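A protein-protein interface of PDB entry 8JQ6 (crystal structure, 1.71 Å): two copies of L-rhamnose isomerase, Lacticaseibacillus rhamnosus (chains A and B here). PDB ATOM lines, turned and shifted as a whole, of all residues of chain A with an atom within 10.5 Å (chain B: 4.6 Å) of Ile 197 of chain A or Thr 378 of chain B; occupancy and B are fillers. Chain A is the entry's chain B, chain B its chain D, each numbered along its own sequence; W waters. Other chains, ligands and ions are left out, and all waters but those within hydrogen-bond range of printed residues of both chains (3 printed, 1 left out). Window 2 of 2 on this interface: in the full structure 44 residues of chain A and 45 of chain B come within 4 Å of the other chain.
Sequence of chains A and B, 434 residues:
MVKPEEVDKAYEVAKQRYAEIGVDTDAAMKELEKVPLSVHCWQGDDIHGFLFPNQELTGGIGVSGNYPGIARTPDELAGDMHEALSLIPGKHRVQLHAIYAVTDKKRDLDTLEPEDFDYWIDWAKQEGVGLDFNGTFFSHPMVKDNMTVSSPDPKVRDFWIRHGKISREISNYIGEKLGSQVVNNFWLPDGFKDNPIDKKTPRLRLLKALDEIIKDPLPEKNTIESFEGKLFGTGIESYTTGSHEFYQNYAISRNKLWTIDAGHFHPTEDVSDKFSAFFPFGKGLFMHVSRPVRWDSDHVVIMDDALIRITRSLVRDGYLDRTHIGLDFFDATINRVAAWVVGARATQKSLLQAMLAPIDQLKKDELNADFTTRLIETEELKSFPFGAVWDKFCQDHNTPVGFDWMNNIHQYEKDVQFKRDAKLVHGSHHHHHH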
ATOM      1  N   MET A 147      17.999 -30.654   6.212  1.00  0.00           N
ATOM      2  CA  MET A 147      17.511 -31.453   5.062  1.00  0.00           C
ATOM      3  C   MET A 147      18.262 -32.784   4.962  1.00  0.00           C
ATOM      4  O   MET A 147      19.419 -32.874   5.419  1.00  0.00           O
ATOM      5  CB  MET A 147      17.650 -30.674   3.754  1.00  0.00           C
ATOM      6  CG  MET A 147      16.742 -29.466   3.695  1.00  0.00           C
ATOM      7  SD  MET A 147      16.921 -28.601   2.133  1.00  0.00           S
ATOM      8  CE  MET A 147      15.796 -27.227   2.378  1.00  0.00           C
ATOM      9  N   GLY A 191      13.185 -28.892   5.591  1.00  0.00           N
ATOM     10  CA  GLY A 191      12.481 -27.609   5.431  1.00  0.00           C
ATOM     11  C   GLY A 191      13.411 -26.432   5.654  1.00  0.00           C
ATOM     12  O   GLY A 191      14.641 -26.624   5.650  1.00  0.00           O
ATOM     13  N   PHE A 192      12.833 -25.253   5.864  1.00  0.00           N
ATOM     14  CA  PHE A 192      13.585 -24.003   6.107  1.00  0.00           C
ATOM     15  C   PHE A 192      13.090 -23.329   7.380  1.00  0.00           C
ATOM     16  O   PHE A 192      11.863 -23.284   7.636  1.00  0.00           O
ATOM     17  CB  PHE A 192      13.407 -23.002   4.968  1.00  0.00           C
ATOM     18  CG  PHE A 192      14.086 -23.368   3.678  1.00  0.00           C
ATOM     19  CD1 PHE A 192      15.447 -23.173   3.512  1.00  0.00           C
ATOM     20  CD2 PHE A 192      13.347 -23.846   2.610  1.00  0.00           C
ATOM     21  CE1 PHE A 192      16.057 -23.472   2.303  1.00  0.00           C
ATOM     22  CE2 PHE A 192      13.962 -24.164   1.410  1.00  0.00           C
ATOM     23  CZ  PHE A 192      15.313 -23.962   1.253  1.00  0.00           C
ATOM     24  N   LYS A 193      14.038 -22.751   8.116  1.00  0.00           N
ATOM     25  CA  LYS A 193      13.742 -21.903   9.283  1.00  0.00           C
ATOM     26  C   LYS A 193      12.994 -20.648   8.826  1.00  0.00           C
ATOM     27  O   LYS A 193      11.978 -20.289   9.458  1.00  0.00           O
ATOM     28  CB  LYS A 193      15.031 -21.520  10.002  1.00  0.00           C
ATOM     29  CG  LYS A 193      14.785 -20.516  11.119  1.00  0.00           C
ATOM     30  CD  LYS A 193      15.939 -20.288  12.028  1.00  0.00           C
ATOM     31  CE  LYS A 193      15.522 -19.346  13.136  1.00  0.00           C
ATOM     32  NZ  LYS A 193      16.439 -19.403  14.289  1.00  0.00           N
ATOM     33  N   ASP A 194      13.489 -19.993   7.779  1.00  0.00           N
ATOM     34  CA  ASP A 194      12.947 -18.686   7.332  1.00  0.00           C
ATOM     35  C   ASP A 194      12.345 -18.872   5.943  1.00  0.00           C
ATOM     36  O   ASP A 194      12.417 -19.988   5.410  1.00  0.00           O
ATOM     37  CB  ASP A 194      14.003 -17.585   7.415  1.00  0.00           C
ATOM     38  CG  ASP A 194      13.457 -16.259   7.926  1.00  0.00           C
ATOM     39  OD1 ASP A 194      14.106 -15.654   8.807  1.00  0.00           O
ATOM     40  OD2 ASP A 194      12.373 -15.861   7.473  1.00  0.00           O
ATOM     41  N   ASN A 195      11.751 -17.810   5.409  1.00  0.00           N
ATOM     42  CA  ASN A 195      10.887 -17.827   4.203  1.00  0.00           C
ATOM     43  C   ASN A 195      11.702 -18.255   2.986  1.00  0.00           C
ATOM     44  O   ASN A 195      12.704 -17.628   2.642  1.00  0.00           O
ATOM     45  CB  ASN A 195      10.232 -16.459   4.006  1.00  0.00           C
ATOM     46  CG  ASN A 195       9.178 -16.191   5.055  1.00  0.00           C
ATOM     47  OD1 ASN A 195       8.359 -17.065   5.335  1.00  0.00           O
ATOM     48  ND2 ASN A 195       9.201 -15.009   5.653  1.00  0.00           N
ATOM     49  N   PRO A 196      11.313 -19.335   2.278  1.00  0.00           N
ATOM     50  CA  PRO A 196      12.050 -19.741   1.091  1.00  0.00           C
ATOM     51  C   PRO A 196      11.649 -18.966  -0.171  1.00  0.00           C
ATOM     52  O   PRO A 196      10.531 -18.461  -0.250  1.00  0.00           O
ATOM     53  CB  PRO A 196      11.660 -21.218   0.948  1.00  0.00           C
ATOM     54  CG  PRO A 196      10.241 -21.248   1.436  1.00  0.00           C
ATOM     55  CD  PRO A 196      10.218 -20.267   2.592  1.00  0.00           C
ATOM     56  N   ILE A 197      12.582 -18.915  -1.120  1.00  0.00           N
ATOM     57  CA  ILE A 197      12.374 -18.361  -2.485  1.00  0.00           C
ATOM     58  C   ILE A 197      11.751 -19.449  -3.363  1.00  0.00           C
ATOM     59  O   ILE A 197      10.784 -19.138  -4.076  1.00  0.00           O
ATOM     60  CB  ILE A 197      13.695 -17.849  -3.074  1.00  0.00           C
ATOM     61  CG1 ILE A 197      14.394 -16.879  -2.115  1.00  0.00           C
ATOM     62  CG2 ILE A 197      13.447 -17.230  -4.444  1.00  0.00           C
ATOM     63  CD1 ILE A 197      13.537 -15.708  -1.698  1.00  0.00           C
ATOM     64  N   ASP A 198      12.296 -20.669  -3.309  1.00  0.00           N
ATOM     65  CA  ASP A 198      11.876 -21.793  -4.189  1.00  0.00           C
ATOM     66  C   ASP A 198      11.179 -22.862  -3.339  1.00  0.00           C
ATOM     67  O   ASP A 198      11.866 -23.564  -2.577  1.00  0.00           O
ATOM     68  CB  ASP A 198      13.065 -22.342  -4.979  1.00  0.00           C
ATOM     69  CG  ASP A 198      12.680 -23.376  -6.021  1.00  0.00           C
ATOM     70  OD1 ASP A 198      11.641 -24.051  -5.827  1.00  0.00           O
ATOM     71  OD2 ASP A 198      13.425 -23.509  -7.014  1.00  0.00           O
ATOM     72  N   LYS A 199       9.856 -22.966  -3.468  1.00  0.00           N
ATOM     73  CA  LYS A 199       9.033 -23.979  -2.755  1.00  0.00           C
ATOM     74  C   LYS A 199       8.857 -25.218  -3.639  1.00  0.00           C
ATOM     75  O   LYS A 199       8.590 -26.318  -3.090  1.00  0.00           O
ATOM     76  CB  LYS A 199       7.671 -23.392  -2.394  1.00  0.00           C
ATOM     77  CG  LYS A 199       7.707 -22.255  -1.385  1.00  0.00           C
ATOM     78  CD  LYS A 199       6.315 -21.745  -1.084  1.00  0.00           C
ATOM     79  CE  LYS A 199       6.287 -20.554  -0.159  1.00  0.00           C
ATOM     80  NZ  LYS A 199       4.890 -20.216   0.193  1.00  0.00           N
ATOM     81  N   LYS A 200       9.012 -25.046  -4.951  1.00  0.00           N
ATOM     82  CA  LYS A 200       8.766 -26.117  -5.958  1.00  0.00           C
ATOM     83  C   LYS A 200       9.885 -27.165  -5.935  1.00  0.00           C
ATOM     84  O   LYS A 200       9.580 -28.375  -5.828  1.00  0.00           O
ATOM     85  CB  LYS A 200       8.649 -25.509  -7.354  1.00  0.00           C
ATOM     86  CG  LYS A 200       8.649 -26.535  -8.482  1.00  0.00           C
ATOM     87  CD  LYS A 200       8.437 -25.952  -9.859  1.00  0.00           C
ATOM     88  CE  LYS A 200       9.582 -25.070 -10.287  1.00  0.00           C
ATOM     89  NZ  LYS A 200       9.412 -24.615 -11.683  1.00  0.00           N
ATOM     90  N   THR A 201      11.135 -26.735  -6.079  1.00  0.00           N
ATOM     91  CA  THR A 201      12.286 -27.629  -6.364  1.00  0.00           C
ATOM     92  C   THR A 201      12.518 -28.590  -5.195  1.00  0.00           C
ATOM     93  O   THR A 201      12.736 -29.774  -5.423  1.00  0.00           O
ATOM     94  CB  THR A 201      13.517 -26.816  -6.770  1.00  0.00           C
ATOM     95  OG1 THR A 201      13.105 -26.003  -7.871  1.00  0.00           O
ATOM     96  CG2 THR A 201      14.700 -27.689  -7.138  1.00  0.00           C
ATOM     97  N   PRO A 202      12.479 -28.149  -3.915  1.00  0.00           N
ATOM     98  CA  PRO A 202      12.640 -29.079  -2.796  1.00  0.00           C
ATOM     99  C   PRO A 202      11.631 -30.231  -2.876  1.00  0.00           C
ATOM    100  O   PRO A 202      12.000 -31.380  -2.629  1.00  0.00           O
ATOM    101  CB  PRO A 202      12.383 -28.200  -1.560  1.00  0.00           C
ATOM    102  CG  PRO A 202      12.791 -26.815  -2.023  1.00  0.00           C
ATOM    103  CD  PRO A 202      12.322 -26.761  -3.462  1.00  0.00           C
ATOM    104  N   ARG A 205      12.592 -32.603  -5.610  1.00  0.00           N
ATOM    105  CA  ARG A 205      13.740 -33.424  -5.144  1.00  0.00           C
ATOM    106  C   ARG A 205      13.186 -34.518  -4.226  1.00  0.00           C
ATOM    107  O   ARG A 205      13.629 -35.671  -4.349  1.00  0.00           O
ATOM    108  CB  ARG A 205      14.819 -32.599  -4.437  1.00  0.00           C
ATOM    109  CG  ARG A 205      15.619 -31.692  -5.361  1.00  0.00           C
ATOM    110  CD  ARG A 205      16.876 -31.134  -4.724  1.00  0.00           C
ATOM    111  NE  ARG A 205      16.604 -30.515  -3.429  1.00  0.00           N
ATOM    112  CZ  ARG A 205      16.452 -29.216  -3.209  1.00  0.00           C
ATOM    113  NH1 ARG A 205      16.573 -28.342  -4.197  1.00  0.00           N
ATOM    114  NH2 ARG A 205      16.193 -28.794  -1.981  1.00  0.00           N
ATOM    115  N   SER A 238       9.314 -22.121   8.962  1.00  0.00           N
ATOM    116  CA  SER A 238       8.717 -21.342   7.844  1.00  0.00           C
ATOM    117  C   SER A 238       8.244 -22.244   6.696  1.00  0.00           C
ATOM    118  O   SER A 238       7.280 -21.867   6.007  1.00  0.00           O
ATOM    119  CB  SER A 238       9.679 -20.286   7.353  1.00  0.00           C
ATOM    120  OG  SER A 238       9.786 -19.258   8.320  1.00  0.00           O
ATOM    121  N   TYR A 239       8.890 -23.387   6.477  1.00  0.00           N
ATOM    122  CA  TYR A 239       8.565 -24.281   5.338  1.00  0.00           C
ATOM    123  C   TYR A 239       8.940 -25.708   5.699  1.00  0.00           C
ATOM    124  O   TYR A 239      10.050 -25.929   6.211  1.00  0.00           O
ATOM    125  CB  TYR A 239       9.317 -23.825   4.089  1.00  0.00           C
ATOM    126  CG  TYR A 239       9.239 -24.716   2.872  1.00  0.00           C
ATOM    127  CD1 TYR A 239       8.267 -24.530   1.901  1.00  0.00           C
ATOM    128  CD2 TYR A 239      10.209 -25.680   2.641  1.00  0.00           C
ATOM    129  CE1 TYR A 239       8.241 -25.300   0.741  1.00  0.00           C
ATOM    130  CE2 TYR A 239      10.194 -26.459   1.495  1.00  0.00           C
ATOM    131  CZ  TYR A 239       9.204 -26.276   0.547  1.00  0.00           C
ATOM    132  OH  TYR A 239       9.219 -27.054  -0.578  1.00  0.00           O
ATOM    133  N   ARG B 316       7.639 -16.862  -8.346  1.00  0.00           N
ATOM    134  CA  ARG B 316       8.982 -17.422  -8.066  1.00  0.00           C
ATOM    135  C   ARG B 316       9.074 -18.843  -8.629  1.00  0.00           C
ATOM    136  O   ARG B 316      10.137 -19.196  -9.143  1.00  0.00           O
ATOM    137  CB  ARG B 316       9.244 -17.414  -6.560  1.00  0.00           C
ATOM    138  CG  ARG B 316       9.497 -16.019  -6.017  1.00  0.00           C
ATOM    139  CD  ARG B 316       9.498 -16.019  -4.515  1.00  0.00           C
ATOM    140  NE  ARG B 316       9.910 -14.741  -3.971  1.00  0.00           N
ATOM    141  CZ  ARG B 316      10.047 -14.506  -2.677  1.00  0.00           C
ATOM    142  NH1 ARG B 316       9.796 -15.468  -1.806  1.00  0.00           N
ATOM    143  NH2 ARG B 316      10.454 -13.323  -2.259  1.00  0.00           N
ATOM    144  N   ASP B 317       7.999 -19.622  -8.543  1.00  0.00           N
ATOM    145  CA  ASP B 317       8.049 -21.065  -8.894  1.00  0.00           C
ATOM    146  C   ASP B 317       7.432 -21.303 -10.281  1.00  0.00           C
ATOM    147  O   ASP B 317       7.336 -22.483 -10.688  1.00  0.00           O
ATOM    148  CB  ASP B 317       7.443 -21.912  -7.777  1.00  0.00           C
ATOM    149  CG  ASP B 317       8.313 -21.932  -6.527  1.00  0.00           C
ATOM    150  OD1 ASP B 317       9.553 -21.844  -6.669  1.00  0.00           O
ATOM    151  OD2 ASP B 317       7.746 -22.001  -5.423  1.00  0.00           O
ATOM    152  N   ILE B 359      15.211 -13.114  -8.946  1.00  0.00           N
ATOM    153  CA  ILE B 359      14.724 -14.445  -8.488  1.00  0.00           C
ATOM    154  C   ILE B 359      15.785 -15.506  -8.785  1.00  0.00           C
ATOM    155  O   ILE B 359      16.023 -16.347  -7.895  1.00  0.00           O
ATOM    156  CB  ILE B 359      13.356 -14.782  -9.106  1.00  0.00           C
ATOM    157  CG1 ILE B 359      12.273 -13.807  -8.639  1.00  0.00           C
ATOM    158  CG2 ILE B 359      12.975 -16.213  -8.784  1.00  0.00           C
ATOM    159  CD1 ILE B 359      10.959 -13.966  -9.364  1.00  0.00           C
ATOM    160  N   LEU B 362      18.583 -15.115  -6.250  1.00  0.00           N
ATOM    161  CA  LEU B 362      18.087 -15.438  -4.886  1.00  0.00           C
ATOM    162  C   LEU B 362      17.994 -16.960  -4.766  1.00  0.00           C
ATOM    163  O   LEU B 362      18.359 -17.493  -3.715  1.00  0.00           O
ATOM    164  CB  LEU B 362      16.746 -14.744  -4.644  1.00  0.00           C
ATOM    165  CG  LEU B 362      16.875 -13.259  -4.296  1.00  0.00           C
ATOM    166  CD1 LEU B 362      15.529 -12.553  -4.332  1.00  0.00           C
ATOM    167  CD2 LEU B 362      17.536 -13.091  -2.936  1.00  0.00           C
ATOM    168  N   LYS B 363      17.558 -17.641  -5.826  1.00  0.00           N
ATOM    169  CA  LYS B 363      17.464 -19.122  -5.820  1.00  0.00           C
ATOM    170  C   LYS B 363      18.860 -19.716  -5.635  1.00  0.00           C
ATOM    171  O   LYS B 363      18.986 -20.641  -4.805  1.00  0.00           O
ATOM    172  CB  LYS B 363      16.764 -19.641  -7.076  1.00  0.00           C
ATOM    173  CG  LYS B 363      15.250 -19.517  -7.031  1.00  0.00           C
ATOM    174  CD  LYS B 363      14.542 -20.192  -8.171  1.00  0.00           C
ATOM    175  CE  LYS B 363      13.043 -20.020  -8.088  1.00  0.00           C
ATOM    176  NZ  LYS B 363      12.367 -20.678  -9.227  1.00  0.00           N
ATOM    177  N   GLU B 366      20.079 -19.267  -2.021  1.00  0.00           N
ATOM    178  CA  GLU B 366      19.314 -20.197  -1.156  1.00  0.00           C
ATOM    179  C   GLU B 366      19.843 -21.629  -1.321  1.00  0.00           C
ATOM    180  O   GLU B 366      19.951 -22.334  -0.305  1.00  0.00           O
ATOM    181  CB  GLU B 366      17.844 -20.105  -1.534  1.00  0.00           C
ATOM    182  CG  GLU B 366      16.967 -21.106  -0.825  1.00  0.00           C
ATOM    183  CD  GLU B 366      15.506 -20.770  -1.026  1.00  0.00           C
ATOM    184  OE1 GLU B 366      14.945 -21.244  -2.020  1.00  0.00           O
ATOM    185  OE2 GLU B 366      14.958 -19.983  -0.218  1.00  0.00           O
ATOM    186  N   ARG B 374      19.727 -13.873   1.641  1.00  0.00           N
ATOM    187  CA  ARG B 374      18.286 -14.023   1.314  1.00  0.00           C
ATOM    188  C   ARG B 374      17.455 -13.094   2.209  1.00  0.00           C
ATOM    189  O   ARG B 374      16.571 -12.394   1.671  1.00  0.00           O
ATOM    190  CB  ARG B 374      17.834 -15.478   1.455  1.00  0.00           C
ATOM    191  CG  ARG B 374      16.402 -15.696   0.995  1.00  0.00           C
ATOM    192  CD  ARG B 374      15.933 -17.098   1.297  1.00  0.00           C
ATOM    193  NE  ARG B 374      15.933 -17.331   2.727  1.00  0.00           N
ATOM    194  CZ  ARG B 374      15.897 -18.526   3.294  1.00  0.00           C
ATOM    195  NH1 ARG B 374      15.831 -19.616   2.549  1.00  0.00           N
ATOM    196  NH2 ARG B 374      15.905 -18.619   4.611  1.00  0.00           N
ATOM    197  N   LEU B 375      17.726 -13.070   3.516  1.00  0.00           N
ATOM    198  CA  LEU B 375      16.937 -12.248   4.471  1.00  0.00           C
ATOM    199  C   LEU B 375      17.177 -10.765   4.163  1.00  0.00           C
ATOM    200  O   LEU B 375      16.194  -9.999   4.059  1.00  0.00           O
ATOM    201  CB  LEU B 375      17.324 -12.585   5.914  1.00  0.00           C
ATOM    202  CG  LEU B 375      16.592 -11.756   6.970  1.00  0.00           C
ATOM    203  CD1 LEU B 375      15.091 -12.021   6.912  1.00  0.00           C
ATOM    204  CD2 LEU B 375      17.132 -12.021   8.368  1.00  0.00           C
ATOM    205  N   ILE B 376      18.437 -10.355   4.041  1.00  0.00           N
ATOM    206  CA  ILE B 376      18.768  -8.916   3.835  1.00  0.00           C
ATOM    207  C   ILE B 376      18.086  -8.452   2.542  1.00  0.00           C
ATOM    208  O   ILE B 376      17.374  -7.438   2.577  1.00  0.00           O
ATOM    209  CB  ILE B 376      20.286  -8.673   3.817  1.00  0.00           C
ATOM    210  CG1 ILE B 376      20.936  -9.018   5.161  1.00  0.00           C
ATOM    211  CG2 ILE B 376      20.579  -7.235   3.412  1.00  0.00           C
ATOM    212  CD1 ILE B 376      22.448  -8.995   5.126  1.00  0.00           C
ATOM    213  N   GLU B 377      18.268  -9.186   1.444  1.00  0.00           N
ATOM    214  CA  GLU B 377      17.816  -8.733   0.103  1.00  0.00           C
ATOM    215  C   GLU B 377      16.288  -8.722   0.022  1.00  0.00           C
ATOM    216  O   GLU B 377      15.742  -7.727  -0.473  1.00  0.00           O
ATOM    217  CB  GLU B 377      18.433  -9.594  -0.993  1.00  0.00           C
ATOM    218  CG  GLU B 377      19.897  -9.298  -1.225  1.00  0.00           C
ATOM    219  CD  GLU B 377      20.409  -9.955  -2.489  1.00  0.00           C
ATOM    220  OE1 GLU B 377      19.563 -10.462  -3.246  1.00  0.00           O
ATOM    221  OE2 GLU B 377      21.638  -9.955  -2.704  1.00  0.00           O
ATOM    222  N   THR B 378      15.606  -9.781   0.467  1.00  0.00           N
ATOM    223  CA  THR B 378      14.121  -9.826   0.439  1.00  0.00           C
ATOM    224  C   THR B 378      13.569  -8.636   1.245  1.00  0.00           C
ATOM    225  O   THR B 378      12.546  -8.060   0.835  1.00  0.00           O
ATOM    226  CB  THR B 378      13.600 -11.196   0.885  1.00  0.00           C
ATOM    227  OG1 THR B 378      14.175 -11.530   2.148  1.00  0.00           O
ATOM    228  CG2 THR B 378      13.921 -12.278  -0.126  1.00  0.00           C
ATOM    229  N   GLU B 379      14.224  -8.259   2.341  1.00  0.00           N
ATOM    230  CA  GLU B 379      13.751  -7.135   3.185  1.00  0.00           C
ATOM    231  C   GLU B 379      14.048  -5.814   2.473  1.00  0.00           C
ATOM    232  O   GLU B 379      13.151  -4.942   2.453  1.00  0.00           O
ATOM    233  CB  GLU B 379      14.355  -7.223   4.587  1.00  0.00           C
ATOM    234  CG  GLU B 379      13.641  -8.249   5.443  1.00  0.00           C
ATOM    235  CD  GLU B 379      12.128  -8.120   5.422  1.00  0.00           C
ATOM    236  OE1 GLU B 379      11.618  -7.070   5.876  1.00  0.00           O
ATOM    237  OE2 GLU B 379      11.460  -9.066   4.955  1.00  0.00           O
ATOM    238  N   GLU B 380      15.236  -5.668   1.884  1.00  0.00           N
ATOM    239  CA  GLU B 380      15.581  -4.415   1.159  1.00  0.00           C
ATOM    240  C   GLU B 380      14.589  -4.211   0.005  1.00  0.00           C
ATOM    241  O   GLU B 380      14.213  -3.057  -0.257  1.00  0.00           O
ATOM    242  CB  GLU B 380      17.035  -4.412   0.680  1.00  0.00           C
ATOM    243  CG  GLU B 380      18.041  -4.260   1.812  1.00  0.00           C
ATOM    244  CD  GLU B 380      17.777  -3.110   2.766  1.00  0.00           C
ATOM    245  OE1 GLU B 380      17.359  -2.021   2.291  1.00  0.00           O
ATOM    246  OE2 GLU B 380      17.995  -3.300   3.984  1.00  0.00           O
ATOM    247  N   LEU B 381      14.167  -5.284  -0.665  1.00  0.00           N
ATOM    248  CA  LEU B 381      13.326  -5.173  -1.882  1.00  0.00           C
ATOM    249  C   LEU B 381      11.952  -4.598  -1.521  1.00  0.00           C
ATOM    250  O   LEU B 381      11.324  -3.973  -2.390  1.00  0.00           O
ATOM    251  CB  LEU B 381      13.214  -6.548  -2.539  1.00  0.00           C
ATOM    252  CG  LEU B 381      14.427  -6.962  -3.371  1.00  0.00           C
ATOM    253  CD1 LEU B 381      14.317  -8.423  -3.781  1.00  0.00           C
ATOM    254  CD2 LEU B 381      14.583  -6.073  -4.596  1.00  0.00           C
ATOM    255  N   LYS B 382      11.502  -4.781  -0.283  1.00  0.00           N
ATOM    256  CA  LYS B 382      10.170  -4.303   0.159  1.00  0.00           C
ATOM    257  C   LYS B 382      10.108  -2.772   0.139  1.00  0.00           C
ATOM    258  O   LYS B 382       8.977  -2.254   0.101  1.00  0.00           O
ATOM    259  CB  LYS B 382       9.833  -4.856   1.543  1.00  0.00           C
ATOM    260  CG  LYS B 382       9.621  -6.362   1.559  1.00  0.00           C
ATOM    261  CD  LYS B 382       9.299  -6.901   2.922  1.00  0.00           C
ATOM    262  CE  LYS B 382       8.844  -8.340   2.865  1.00  0.00           C
ATOM    263  NZ  LYS B 382       8.826  -8.939   4.218  1.00  0.00           N
HETATM  264  O   HOH W   1       8.072 -17.900  -1.899  1.00  0.00           O
HETATM  265  O   HOH W   2       8.123 -19.615  -4.126  1.00  0.00           O
HETATM  266  O   HOH W   3      14.566 -23.958  -2.179  1.00  0.00           O
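Ile 197 of chain A touches just these residues of chain B: Arg 316 (3.4 Å), Asp 317 (3.9 Å), Lys 363 (3.9 Å), Glu 366 (2.8 Å), Arg 374 (3.7 Å) and Thr 378 (3.8 Å). Thr 378 of chain B touches one residue of chain A. No residue of chain A comes within 4 Å of Ile 359 of chain B. No residue of chain A comes within 4 Å of Leu 362 of chain B. Of the printed residues of chain A, Lys 363 of chain B touches Ile 197 (3.9 Å) and Asp 198 (3.7 Å). Leu 381 of chain B touches none of the printed residues of chain A. Of the printed residues of chain A, Glu 366 of chain B touches Phe 192, Pro 196, Ile 197 and Asp 198. Of the printed residues of chain B, Lys 200 of chain A touches Asp 317 (3.1 Å). Of the printed residues of chain B, Asn 195 of chain A touches Arg 374. Printed residues of chain B within 4 Å of Asp 198 of chain A: Asp 317, Lys 363 and Glu 366. Of the printed residues of chain B, Phe 192 of chain A touches Glu 366 (3.9 Å) and Arg 374 (3.7 Å). Arg 205 of chain A touches none of the printed residues of chain B. The nearest residue of chain B that does not touch Ile 197 of chain A is Leu 362 of chain B (4.1 Å). The nearest residue of chain A that does not touch Thr 378 of chain B is Asn 195 of chain A (6.1 Å). The nearest printed residue of chain B that does not touch Phe 192 of chain A is Lys 363 of chain B (7.8 Å).
No position is printed for both chains.
Printed residues of chain A that touch a printed residue of chain B: Phe 192, Asp 194, Asn 195, Pro 196, Ile 197, Asp 198, Lys 199 and Lys 200. Hydrophobic or aromatic side chains of chain A within 4 Å of the printed part of chain B: Phe 192, Pro 196 and Ile 197. Among the printed residues, 17 pairs touch across the chains.
O of Asn 195 of chain A lies within hydrogen-bond range of NE of Arg 374 of chain B (3.2 Å). O of Pro 196 of chain A lies within hydrogen-bond range of NH1 of Arg 316 of chain B. The side-chain carboxylate (OE2) of Glu 366 of chain B lies within hydrogen-bond range of the backbone NH (N) of Ile 197 of chain A (2.8 Å). NZ of Lys 363 of chain B is in salt-bridge range of OD2 of Asp 198 of chain A. The backbone NH (N) of Asp 198 of chain A sits at hydrogen-bond distance from the side-chain carboxylate (OE1) of Glu 366 of chain B, at 3.0 Å. OD2 of Asp 317 of chain B sits at hydrogen-bond distance from N of Lys 199 of chain A, 3.0 Å away. The side-chain amino group (NZ) of Lys 200 of chain A sits at hydrogen-bond distance from the backbone carbonyl oxygen (O) of Asp 317 of chain B, 3.1 Å away. The side-chain carboxylate of Asp 198 of chain A lies close to the side-chain carboxylate of Asp 317 of chain B.
Phe 192 of chain A touches Glu 366 of chain B (CZ to CG, 3.9 Å). Arg 374 of chain B touches Phe 192 of chain A (NH1 to CD1, 3.7 Å). Arg 374 of chain B touches Asp 194 of chain A. Pro 196 of chain A touches Glu 366 of chain B. CB of Arg 316 of chain B touches O of Ile 197 of chain A, at 3.4 Å. O of Ile 197 of chain A touches OD1 of Asp 317 of chain B, at 3.9 Å. Lys 363 of chain B touches Ile 197 of chain A (CG to CG2, 3.9 Å). Ile 197 of chain A touches Arg 374 of chain B. Ile 197 of chain A touches Thr 378 of chain B.
The backbone carbonyl oxygen (O) of Phe 192 of chain A sits at hydrogen-bond distance from the backbone NH (N) of Ser 238 of chain A. The backbone NH (N) of Phe 192 of chain A lies within hydrogen-bond range of the backbone carbonyl oxygen (O) of Tyr 239 of chain A (2.9 Å). OD1 of Asp 198 of chain A lies within hydrogen-bond range of N of Lys 200 of chain A, at 2.9 Å. The backbone carbonyl oxygen (O) of Arg 316 of chain B sits at hydrogen-bond distance from the side-chain amino group (NZ) of Lys 363 of chain B (2.7 Å). The guanidinium group of Arg 374 of chain B lies within salt-bridge range of the side-chain carboxylate of Glu 366 of chain B (2.9 Å). The backbone carbonyl oxygen (O) of Leu 375 of chain B is in hydrogen-bond range of the side-chain hydroxyl (OG1) of Thr 378 of chain B (3.2 Å).
Water W2 bridges the backbone carbonyl oxygen (O) of Ile 197 of chain A (2.7 Å) and the side-chain carboxylate (OD2) of Asp 317 of chain B (2.7 Å). Water W3 lies within hydrogen-bond range of OE1 of Glu 366 of chain B (2.7 Å) and O of Asp 198 of chain A (2.8 Å). Water W1 lies within hydrogen-bond range of the guanidinium group (NH1) of Arg 316 of chain B (3.0 Å) and the backbone carbonyl oxygen (O) of Pro 196 of chain A (3.0 Å).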
